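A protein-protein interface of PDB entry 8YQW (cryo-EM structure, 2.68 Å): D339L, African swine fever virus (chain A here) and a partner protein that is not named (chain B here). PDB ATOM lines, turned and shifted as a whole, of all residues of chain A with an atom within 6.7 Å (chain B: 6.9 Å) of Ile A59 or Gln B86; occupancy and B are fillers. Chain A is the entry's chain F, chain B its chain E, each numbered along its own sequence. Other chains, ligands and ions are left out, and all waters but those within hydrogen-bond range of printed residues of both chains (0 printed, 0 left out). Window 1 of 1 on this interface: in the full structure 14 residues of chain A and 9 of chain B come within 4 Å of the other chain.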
ATOM      1  N   ASP A  15       6.576   2.337   8.271  1.00  0.00           N
ATOM      2  CA  ASP A  15       7.571   1.658   9.098  1.00  0.00           C
ATOM      3  C   ASP A  15       8.533   0.923   8.176  1.00  0.00           C
ATOM      4  O   ASP A  15       8.349  -0.267   7.888  1.00  0.00           O
ATOM      5  CB  ASP A  15       6.913   0.703  10.088  1.00  0.00           C
ATOM      6  CG  ASP A  15       7.868   0.228  11.159  1.00  0.00           C
ATOM      7  OD1 ASP A  15       8.974   0.796  11.262  1.00  0.00           O
ATOM      8  OD2 ASP A  15       7.509  -0.705  11.905  1.00  0.00           O
ATOM      9  N   PRO A  16       9.570   1.605   7.688  1.00  0.00           N
ATOM     10  CA  PRO A  16      10.493   0.958   6.743  1.00  0.00           C
ATOM     11  C   PRO A  16      11.217  -0.247   7.316  1.00  0.00           C
ATOM     12  O   PRO A  16      11.555  -1.166   6.563  1.00  0.00           O
ATOM     13  CB  PRO A  16      11.466   2.090   6.387  1.00  0.00           C
ATOM     14  CG  PRO A  16      10.739   3.342   6.720  1.00  0.00           C
ATOM     15  CD  PRO A  16       9.920   3.014   7.918  1.00  0.00           C
ATOM     16  N   THR A  17      11.472  -0.271   8.626  1.00  0.00           N
ATOM     17  CA  THR A  17      12.185  -1.397   9.220  1.00  0.00           C
ATOM     18  C   THR A  17      11.351  -2.670   9.167  1.00  0.00           C
ATOM     19  O   THR A  17      11.848  -3.736   8.788  1.00  0.00           O
ATOM     20  CB  THR A  17      12.568  -1.071  10.662  1.00  0.00           C
ATOM     21  OG1 THR A  17      13.143   0.240  10.721  1.00  0.00           O
ATOM     22  CG2 THR A  17      13.578  -2.082  11.177  1.00  0.00           C
ATOM     23  N   PRO A  56      14.439   0.348  -4.637  1.00  0.00           N
ATOM     24  CA  PRO A  56      14.813   0.248  -3.225  1.00  0.00           C
ATOM     25  C   PRO A  56      13.892   1.103  -2.373  1.00  0.00           C
ATOM     26  O   PRO A  56      13.226   2.016  -2.865  1.00  0.00           O
ATOM     27  CB  PRO A  56      16.250   0.777  -3.199  1.00  0.00           C
ATOM     28  CG  PRO A  56      16.746   0.603  -4.578  1.00  0.00           C
ATOM     29  CD  PRO A  56      15.567   0.782  -5.477  1.00  0.00           C
ATOM     30  N   CYS A  57      13.845   0.794  -1.083  1.00  0.00           N
ATOM     31  CA  CYS A  57      13.047   1.609  -0.177  1.00  0.00           C
ATOM     32  C   CYS A  57      13.811   2.871   0.191  1.00  0.00           C
ATOM     33  O   CYS A  57      14.614   2.865   1.128  1.00  0.00           O
ATOM     34  CB  CYS A  57      12.670   0.820   1.076  1.00  0.00           C
ATOM     35  SG  CYS A  57      11.591   1.710   2.219  1.00  0.00           S
ATOM     36  N   PHE A  58      13.577   3.955  -0.543  1.00  0.00           N
ATOM     37  CA  PHE A  58      14.204   5.221  -0.213  1.00  0.00           C
ATOM     38  C   PHE A  58      13.581   5.800   1.050  1.00  0.00           C
ATOM     39  O   PHE A  58      12.492   5.411   1.469  1.00  0.00           O
ATOM     40  CB  PHE A  58      14.052   6.222  -1.356  1.00  0.00           C
ATOM     41  CG  PHE A  58      14.390   5.671  -2.707  1.00  0.00           C
ATOM     42  CD1 PHE A  58      15.703   5.585  -3.125  1.00  0.00           C
ATOM     43  CD2 PHE A  58      13.392   5.263  -3.569  1.00  0.00           C
ATOM     44  CE1 PHE A  58      16.011   5.088  -4.369  1.00  0.00           C
ATOM     45  CE2 PHE A  58      13.697   4.770  -4.813  1.00  0.00           C
ATOM     46  CZ  PHE A  58      15.008   4.681  -5.213  1.00  0.00           C
ATOM     47  N   ILE A  59      14.289   6.745   1.659  1.00  0.00           N
ATOM     48  CA  ILE A  59      13.808   7.460   2.835  1.00  0.00           C
ATOM     49  C   ILE A  59      13.409   8.859   2.396  1.00  0.00           C
ATOM     50  O   ILE A  59      14.154   9.519   1.663  1.00  0.00           O
ATOM     51  CB  ILE A  59      14.873   7.508   3.944  1.00  0.00           C
ATOM     52  CG1 ILE A  59      15.297   6.093   4.329  1.00  0.00           C
ATOM     53  CG2 ILE A  59      14.347   8.247   5.154  1.00  0.00           C
ATOM     54  CD1 ILE A  59      14.163   5.235   4.810  1.00  0.00           C
ATOM     55  N   MET A  60      12.227   9.300   2.824  1.00  0.00           N
ATOM     56  CA  MET A  60      11.729  10.610   2.428  1.00  0.00           C
ATOM     57  C   MET A  60      12.716  11.692   2.830  1.00  0.00           C
ATOM     58  O   MET A  60      13.202  11.721   3.963  1.00  0.00           O
ATOM     59  CB  MET A  60      10.366  10.875   3.060  1.00  0.00           C
ATOM     60  CG  MET A  60       9.324   9.829   2.746  1.00  0.00           C
ATOM     61  SD  MET A  60       7.716  10.255   3.420  1.00  0.00           S
ATOM     62  CE  MET A  60       6.687   9.064   2.581  1.00  0.00           C
ATOM     63  N   ARG A  61      13.008  12.587   1.893  1.00  0.00           N
ATOM     64  CA  ARG A  61      14.094  13.542   2.034  1.00  0.00           C
ATOM     65  C   ARG A  61      13.631  14.930   2.440  1.00  0.00           C
ATOM     66  O   ARG A  61      14.408  15.675   3.042  1.00  0.00           O
ATOM     67  CB  ARG A  61      14.867  13.634   0.713  1.00  0.00           C
ATOM     68  CG  ARG A  61      16.208  14.316   0.803  1.00  0.00           C
ATOM     69  CD  ARG A  61      16.746  14.647  -0.576  1.00  0.00           C
ATOM     70  NE  ARG A  61      15.877  15.571  -1.296  1.00  0.00           N
ATOM     71  CZ  ARG A  61      15.861  16.884  -1.118  1.00  0.00           C
ATOM     72  NH1 ARG A  61      16.647  17.471  -0.233  1.00  0.00           N
ATOM     73  NH2 ARG A  61      15.032  17.627  -1.844  1.00  0.00           N
ATOM     74  N   THR A  62      12.387  15.293   2.148  1.00  0.00           N
ATOM     75  CA  THR A  62      11.913  16.653   2.345  1.00  0.00           C
ATOM     76  C   THR A  62      11.146  16.839   3.646  1.00  0.00           C
ATOM     77  O   THR A  62      10.525  17.888   3.838  1.00  0.00           O
ATOM     78  CB  THR A  62      11.041  17.078   1.163  1.00  0.00           C
ATOM     79  OG1 THR A  62      10.027  16.093   0.942  1.00  0.00           O
ATOM     80  CG2 THR A  62      11.881  17.215  -0.089  1.00  0.00           C
ATOM     81  N   ASN A  63      11.170  15.853   4.539  1.00  0.00           N
ATOM     82  CA  ASN A  63      10.532  15.987   5.838  1.00  0.00           C
ATOM     83  C   ASN A  63      11.305  15.159   6.853  1.00  0.00           C
ATOM     84  O   ASN A  63      12.093  14.281   6.497  1.00  0.00           O
ATOM     85  CB  ASN A  63       9.055  15.575   5.793  1.00  0.00           C
ATOM     86  CG  ASN A  63       8.840  14.213   5.169  1.00  0.00           C
ATOM     87  OD1 ASN A  63       9.746  13.390   5.115  1.00  0.00           O
ATOM     88  ND2 ASN A  63       7.634  13.976   4.680  1.00  0.00           N
ATOM     89  N   SER A  65      10.220  12.945   9.013  1.00  0.00           N
ATOM     90  CA  SER A  65       9.383  11.863   9.511  1.00  0.00           C
ATOM     91  C   SER A  65      10.093  10.518   9.539  1.00  0.00           C
ATOM     92  O   SER A  65       9.675   9.632  10.291  1.00  0.00           O
ATOM     93  CB  SER A  65       8.113  11.750   8.664  1.00  0.00           C
ATOM     94  OG  SER A  65       8.366  11.086   7.441  1.00  0.00           O
ATOM     95  N   GLY A  66      11.148  10.342   8.748  1.00  0.00           N
ATOM     96  CA  GLY A  66      11.859   9.085   8.707  1.00  0.00           C
ATOM     97  C   GLY A  66      11.167   7.989   7.932  1.00  0.00           C
ATOM     98  O   GLY A  66      11.660   6.854   7.923  1.00  0.00           O
ATOM     99  N   ARG A  67      10.049   8.288   7.283  1.00  0.00           N
ATOM    100  CA  ARG A  67       9.288   7.300   6.544  1.00  0.00           C
ATOM    101  C   ARG A  67       9.931   7.045   5.185  1.00  0.00           C
ATOM    102  O   ARG A  67      10.821   7.772   4.742  1.00  0.00           O
ATOM    103  CB  ARG A  67       7.842   7.760   6.387  1.00  0.00           C
ATOM    104  CG  ARG A  67       7.111   7.895   7.708  1.00  0.00           C
ATOM    105  CD  ARG A  67       5.922   8.822   7.600  1.00  0.00           C
ATOM    106  NE  ARG A  67       4.848   8.243   6.806  1.00  0.00           N
ATOM    107  CZ  ARG A  67       4.125   8.919   5.924  1.00  0.00           C
ATOM    108  NH1 ARG A  67       4.329  10.207   5.706  1.00  0.00           N
ATOM    109  NH2 ARG A  67       3.172   8.286   5.246  1.00  0.00           N
ATOM    110  N   GLY A  68       9.474   5.983   4.520  1.00  0.00           N
ATOM    111  CA  GLY A  68      10.038   5.565   3.260  1.00  0.00           C
ATOM    112  C   GLY A  68       9.033   5.649   2.122  1.00  0.00           C
ATOM    113  O   GLY A  68       7.848   5.921   2.318  1.00  0.00           O
ATOM    114  N   TYR A  69       9.532   5.403   0.916  1.00  0.00           N
ATOM    115  CA  TYR A  69       8.678   5.315  -0.256  1.00  0.00           C
ATOM    116  C   TYR A  69       9.324   4.365  -1.250  1.00  0.00           C
ATOM    117  O   TYR A  69      10.528   4.112  -1.204  1.00  0.00           O
ATOM    118  CB  TYR A  69       8.428   6.688  -0.887  1.00  0.00           C
ATOM    119  CG  TYR A  69       9.667   7.361  -1.423  1.00  0.00           C
ATOM    120  CD1 TYR A  69      10.503   8.079  -0.587  1.00  0.00           C
ATOM    121  CD2 TYR A  69       9.991   7.289  -2.767  1.00  0.00           C
ATOM    122  CE1 TYR A  69      11.631   8.698  -1.070  1.00  0.00           C
ATOM    123  CE2 TYR A  69      11.117   7.904  -3.258  1.00  0.00           C
ATOM    124  CZ  TYR A  69      11.932   8.608  -2.407  1.00  0.00           C
ATOM    125  OH  TYR A  69      13.060   9.222  -2.898  1.00  0.00           O
ATOM    126  N   ARG B  78      23.323  12.162   8.648  1.00  0.00           N
ATOM    127  CA  ARG B  78      22.048  11.761   8.064  1.00  0.00           C
ATOM    128  C   ARG B  78      21.684  10.332   8.441  1.00  0.00           C
ATOM    129  O   ARG B  78      20.525  10.041   8.752  1.00  0.00           O
ATOM    130  CB  ARG B  78      22.109  11.920   6.547  1.00  0.00           C
ATOM    131  CG  ARG B  78      20.906  11.391   5.811  1.00  0.00           C
ATOM    132  CD  ARG B  78      19.705  12.304   5.953  1.00  0.00           C
ATOM    133  NE  ARG B  78      18.654  11.921   5.021  1.00  0.00           N
ATOM    134  CZ  ARG B  78      17.365  12.168   5.198  1.00  0.00           C
ATOM    135  NH1 ARG B  78      16.925  12.810   6.265  1.00  0.00           N
ATOM    136  NH2 ARG B  78      16.495  11.753   4.282  1.00  0.00           N
ATOM    137  N   VAL B  80      22.635   8.645  11.151  1.00  0.00           N
ATOM    138  CA  VAL B  80      22.264   8.600  12.561  1.00  0.00           C
ATOM    139  C   VAL B  80      20.884   9.204  12.772  1.00  0.00           C
ATOM    140  O   VAL B  80      20.071   8.670  13.532  1.00  0.00           O
ATOM    141  CB  VAL B  80      23.332   9.300  13.423  1.00  0.00           C
ATOM    142  CG1 VAL B  80      22.852   9.442  14.851  1.00  0.00           C
ATOM    143  CG2 VAL B  80      24.621   8.520  13.389  1.00  0.00           C
ATOM    144  N   ALA B  81      20.588  10.319  12.099  1.00  0.00           N
ATOM    145  CA  ALA B  81      19.287  10.958  12.267  1.00  0.00           C
ATOM    146  C   ALA B  81      18.156  10.069  11.766  1.00  0.00           C
ATOM    147  O   ALA B  81      17.127   9.922  12.436  1.00  0.00           O
ATOM    148  CB  ALA B  81      19.269  12.304  11.545  1.00  0.00           C
ATOM    149  N   VAL B  82      18.331   9.465  10.588  1.00  0.00           N
ATOM    150  CA  VAL B  82      17.299   8.591  10.039  1.00  0.00           C
ATOM    151  C   VAL B  82      17.092   7.382  10.939  1.00  0.00           C
ATOM    152  O   VAL B  82      15.954   6.992  11.230  1.00  0.00           O
ATOM    153  CB  VAL B  82      17.663   8.176   8.602  1.00  0.00           C
ATOM    154  CG1 VAL B  82      16.784   7.033   8.138  1.00  0.00           C
ATOM    155  CG2 VAL B  82      17.532   9.358   7.666  1.00  0.00           C
ATOM    156  N   ARG B  83      18.187   6.774  11.404  1.00  0.00           N
ATOM    157  CA  ARG B  83      18.069   5.611  12.274  1.00  0.00           C
ATOM    158  C   ARG B  83      17.400   5.970  13.594  1.00  0.00           C
ATOM    159  O   ARG B  83      16.591   5.199  14.114  1.00  0.00           O
ATOM    160  CB  ARG B  83      19.445   5.001  12.519  1.00  0.00           C
ATOM    161  CG  ARG B  83      19.406   3.690  13.266  1.00  0.00           C
ATOM    162  CD  ARG B  83      18.469   2.714  12.590  1.00  0.00           C
ATOM    163  NE  ARG B  83      18.125   1.598  13.461  1.00  0.00           N
ATOM    164  CZ  ARG B  83      17.033   0.860  13.330  1.00  0.00           C
ATOM    165  NH1 ARG B  83      16.158   1.088  12.366  1.00  0.00           N
ATOM    166  NH2 ARG B  83      16.815  -0.131  14.187  1.00  0.00           N
ATOM    167  N   ALA B  84      17.727   7.137  14.152  1.00  0.00           N
ATOM    168  CA  ALA B  84      17.113   7.557  15.405  1.00  0.00           C
ATOM    169  C   ALA B  84      15.620   7.799  15.240  1.00  0.00           C
ATOM    170  O   ALA B  84      14.825   7.412  16.103  1.00  0.00           O
ATOM    171  CB  ALA B  84      17.808   8.810  15.931  1.00  0.00           C
ATOM    172  N   GLN B  85      15.215   8.432  14.138  1.00  0.00           N
ATOM    173  CA  GLN B  85      13.789   8.638  13.905  1.00  0.00           C
ATOM    174  C   GLN B  85      13.061   7.312  13.713  1.00  0.00           C
ATOM    175  O   GLN B  85      11.958   7.113  14.236  1.00  0.00           O
ATOM    176  CB  GLN B  85      13.581   9.550  12.699  1.00  0.00           C
ATOM    177  CG  GLN B  85      12.137   9.922  12.463  1.00  0.00           C
ATOM    178  CD  GLN B  85      11.592  10.831  13.535  1.00  0.00           C
ATOM    179  OE1 GLN B  85      12.124  11.909  13.781  1.00  0.00           O
ATOM    180  NE2 GLN B  85      10.523  10.397  14.186  1.00  0.00           N
ATOM    181  N   GLN B  86      13.670   6.383  12.976  1.00  0.00           N
ATOM    182  CA  GLN B  86      13.038   5.085  12.773  1.00  0.00           C
ATOM    183  C   GLN B  86      12.967   4.281  14.066  1.00  0.00           C
ATOM    184  O   GLN B  86      12.029   3.501  14.253  1.00  0.00           O
ATOM    185  CB  GLN B  86      13.785   4.312  11.694  1.00  0.00           C
ATOM    186  CG  GLN B  86      13.569   4.878  10.310  1.00  0.00           C
ATOM    187  CD  GLN B  86      14.417   4.196   9.276  1.00  0.00           C
ATOM    188  OE1 GLN B  86      15.274   3.378   9.601  1.00  0.00           O
ATOM    189  NE2 GLN B  86      14.187   4.526   8.016  1.00  0.00           N
ATOM    190  N   LEU B  87      13.948   4.444  14.956  1.00  0.00           N
ATOM    191  CA  LEU B  87      13.857   3.839  16.281  1.00  0.00           C
ATOM    192  C   LEU B  87      12.743   4.476  17.097  1.00  0.00           C
ATOM    193  O   LEU B  87      12.052   3.790  17.857  1.00  0.00           O
ATOM    194  CB  LEU B  87      15.192   3.967  17.009  1.00  0.00           C
ATOM    195  CG  LEU B  87      16.272   2.968  16.609  1.00  0.00           C
ATOM    196  CD1 LEU B  87      17.646   3.533  16.900  1.00  0.00           C
ATOM    197  CD2 LEU B  87      16.066   1.654  17.333  1.00  0.00           C
ATOM    198  N   ALA B  88      12.561   5.790  16.959  1.00  0.00           N
ATOM    199  CA  ALA B  88      11.421   6.443  17.589  1.00  0.00           C
ATOM    200  C   ALA B  88      10.105   5.917  17.035  1.00  0.00           C
ATOM    201  O   ALA B  88       9.078   5.968  17.720  1.00  0.00           O
ATOM    202  CB  ALA B  88      11.511   7.957  17.404  1.00  0.00           C
ATOM    203  N   ILE B  89      10.110   5.412  15.803  1.00  0.00           N
ATOM    204  CA  ILE B  89       8.907   4.793  15.249  1.00  0.00           C
ATOM    205  C   ILE B  89       8.776   3.348  15.721  1.00  0.00           C
ATOM    206  O   ILE B  89       7.760   2.956  16.305  1.00  0.00           O
ATOM    207  CB  ILE B  89       8.908   4.874  13.712  1.00  0.00           C
ATOM    208  CG1 ILE B  89       8.772   6.320  13.239  1.00  0.00           C
ATOM    209  CG2 ILE B  89       7.790   4.024  13.138  1.00  0.00           C
ATOM    210  CD1 ILE B  89       8.978   6.486  11.745  1.00  0.00           C
ATOM    211  N   ASN B  90       9.801   2.533  15.473  1.00  0.00           N
ATOM    212  CA  ASN B  90       9.718   1.098  15.727  1.00  0.00           C
ATOM    213  C   ASN B  90      10.272   0.719  17.099  1.00  0.00           C
ATOM    214  O   ASN B  90       9.552   0.163  17.935  1.00  0.00           O
ATOM    215  CB  ASN B  90      10.458   0.332  14.627  1.00  0.00           C
ATOM    216  CG  ASN B  90       9.997  -1.104  14.506  1.00  0.00           C
ATOM    217  OD1 ASN B  90       9.090  -1.536  15.215  1.00  0.00           O
ATOM    218  ND2 ASN B  90      10.621  -1.853  13.608  1.00  0.00           N
ATOM    219  N   GLY B  91      11.548   1.012  17.342  1.00  0.00           N
ATOM    220  CA  GLY B  91      12.201   0.630  18.574  1.00  0.00           C
ATOM    221  C   GLY B  91      12.943  -0.687  18.528  1.00  0.00           C
ATOM    222  O   GLY B  91      13.599  -1.044  19.514  1.00  0.00           O
ATOM    223  N   SER B  92      12.871  -1.419  17.419  1.00  0.00           N
ATOM    224  CA  SER B  92      13.519  -2.721  17.312  1.00  0.00           C
ATOM    225  C   SER B  92      14.960  -2.549  16.849  1.00  0.00           C
ATOM    226  O   SER B  92      15.207  -2.062  15.742  1.00  0.00           O
ATOM    227  CB  SER B  92      12.750  -3.616  16.344  1.00  0.00           C
ATOM    228  OG  SER B  92      13.509  -4.761  16.002  1.00  0.00           O
ATOM    229  N   PRO B 102      16.903   7.398  21.538  1.00  0.00           N
ATOM    230  CA  PRO B 102      17.090   6.908  20.165  1.00  0.00           C
ATOM    231  C   PRO B 102      18.388   7.382  19.548  1.00  0.00           C
ATOM    232  O   PRO B 102      18.990   6.657  18.748  1.00  0.00           O
ATOM    233  CB  PRO B 102      15.875   7.470  19.416  1.00  0.00           C
ATOM    234  CG  PRO B 102      14.936   7.961  20.471  1.00  0.00           C
ATOM    235  CD  PRO B 102      15.773   8.333  21.641  1.00  0.00           C
ATOM    236  N   PRO B 116      21.035  -0.655   9.888  1.00  0.00           N
ATOM    237  CA  PRO B 116      20.372  -1.274   8.728  1.00  0.00           C
ATOM    238  C   PRO B 116      20.005  -0.262   7.644  1.00  0.00           C
ATOM    239  O   PRO B 116      18.844  -0.126   7.251  1.00  0.00           O
ATOM    240  CB  PRO B 116      19.135  -1.908   9.370  1.00  0.00           C
ATOM    241  CG  PRO B 116      18.787  -0.961  10.456  1.00  0.00           C
ATOM    242  CD  PRO B 116      20.081  -0.379  10.974  1.00  0.00           C
ATOM    243  N   LEU B 117      21.010   0.453   7.146  1.00  0.00           N
ATOM    244  CA  LEU B 117      20.809   1.470   6.127  1.00  0.00           C
ATOM    245  C   LEU B 117      21.926   1.372   5.100  1.00  0.00           C
ATOM    246  O   LEU B 117      22.979   0.788   5.358  1.00  0.00           O
ATOM    247  CB  LEU B 117      20.770   2.878   6.734  1.00  0.00           C
ATOM    248  CG  LEU B 117      19.673   3.180   7.755  1.00  0.00           C
ATOM    249  CD1 LEU B 117      19.900   4.533   8.397  1.00  0.00           C
ATOM    250  CD2 LEU B 117      18.313   3.126   7.101  1.00  0.00           C
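The backbone carbonyl oxygen (O) of Met A60 sits at hydrogen-bond distance from the guanidinium group (NH2) of Arg B78, at 3.3 Å. The side-chain amide nitrogen (NE2) of Gln B86 sits at hydrogen-bond distance from the backbone carbonyl oxygen (O) of Gly A66, at 3.4 Å.
The backbone carbonyl oxygen of Ser B92 sits at hydrogen-bond distance from the guanidinium group of Arg B83, at 3.0 Å. O of Arg A67 sits at hydrogen-bond distance from N of Met A60 (2.8 Å). OG of Ser A65 lies close to N of Arg A67 (3.3 Å).
Among the printed residues, merely in contact across the chains: Asp A15 with Ile B89 (3.9 Å), Asp A15 with Asn B90 (3.6 Å), Pro A16 with Gln B86 (3.9 Å), Thr A17 with Arg B83 (3.5 Å), Thr A17 with Gln B86 (3.96 Å), Thr A17 with Asn B90 (3.6 Å), Ile A59 with Gln B86 (3.3 Å), Arg A61 with Arg B78 (3.7 Å), Ser A65 with Gln B85 (3.3 Å), Ser A65 with Ile B89 (3.5 Å) and Gly A66 with Gln B85 (3.9 Å).
Ile A59 touches just one residue of chain B: Gln B86. Of the printed residues of chain B, Arg A61 touches Arg B78. Of the printed residues of chain A, Arg B78 touches Met A60 (3.3 Å) and Arg A61 (3.7 Å). Of the printed residues of chain A, Gln B85 touches Ser A65 (3.3 Å) and Gly A66 (3.9 Å). Of chain A, only Pro A16 (3.9 Å), Thr A17 (3.96 Å), Ile A59 (3.3 Å) and Gly A66 (3.4 Å) come within 4 Å of Gln B86. Printed residues of chain A within 4 Å of Ile B89: Asp A15 and Ser A65. Of the printed residues of chain A, Asn B90 touches Asp A15 (3.6 Å) and Thr A17 (3.6 Å). The nearest residue of chain B that does not touch Ile A59 is Val B82 (4.04 Å). The nearest residue of chain A that does not touch Gln B86 is Asp A15 (5.1 Å).
Of the 17 printed residues of chain B, 6 touch a printed residue of chain A. Of the 16 printed residues of chain A, 8 touch a printed residue of chain B. Hydrophobic or aromatic side chains of chain A that line the printed part of chain B: Pro A16 and Ile A59. Along chain A the printed residues that touch a printed residue of chain B span positions 15 to 66. Among the printed residues, 13 pairs touch across the chains. Among the printed residues, no Asp or Glu carboxylate lies within 4 Å of a Lys or Arg side-chain nitrogen of the other chain.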
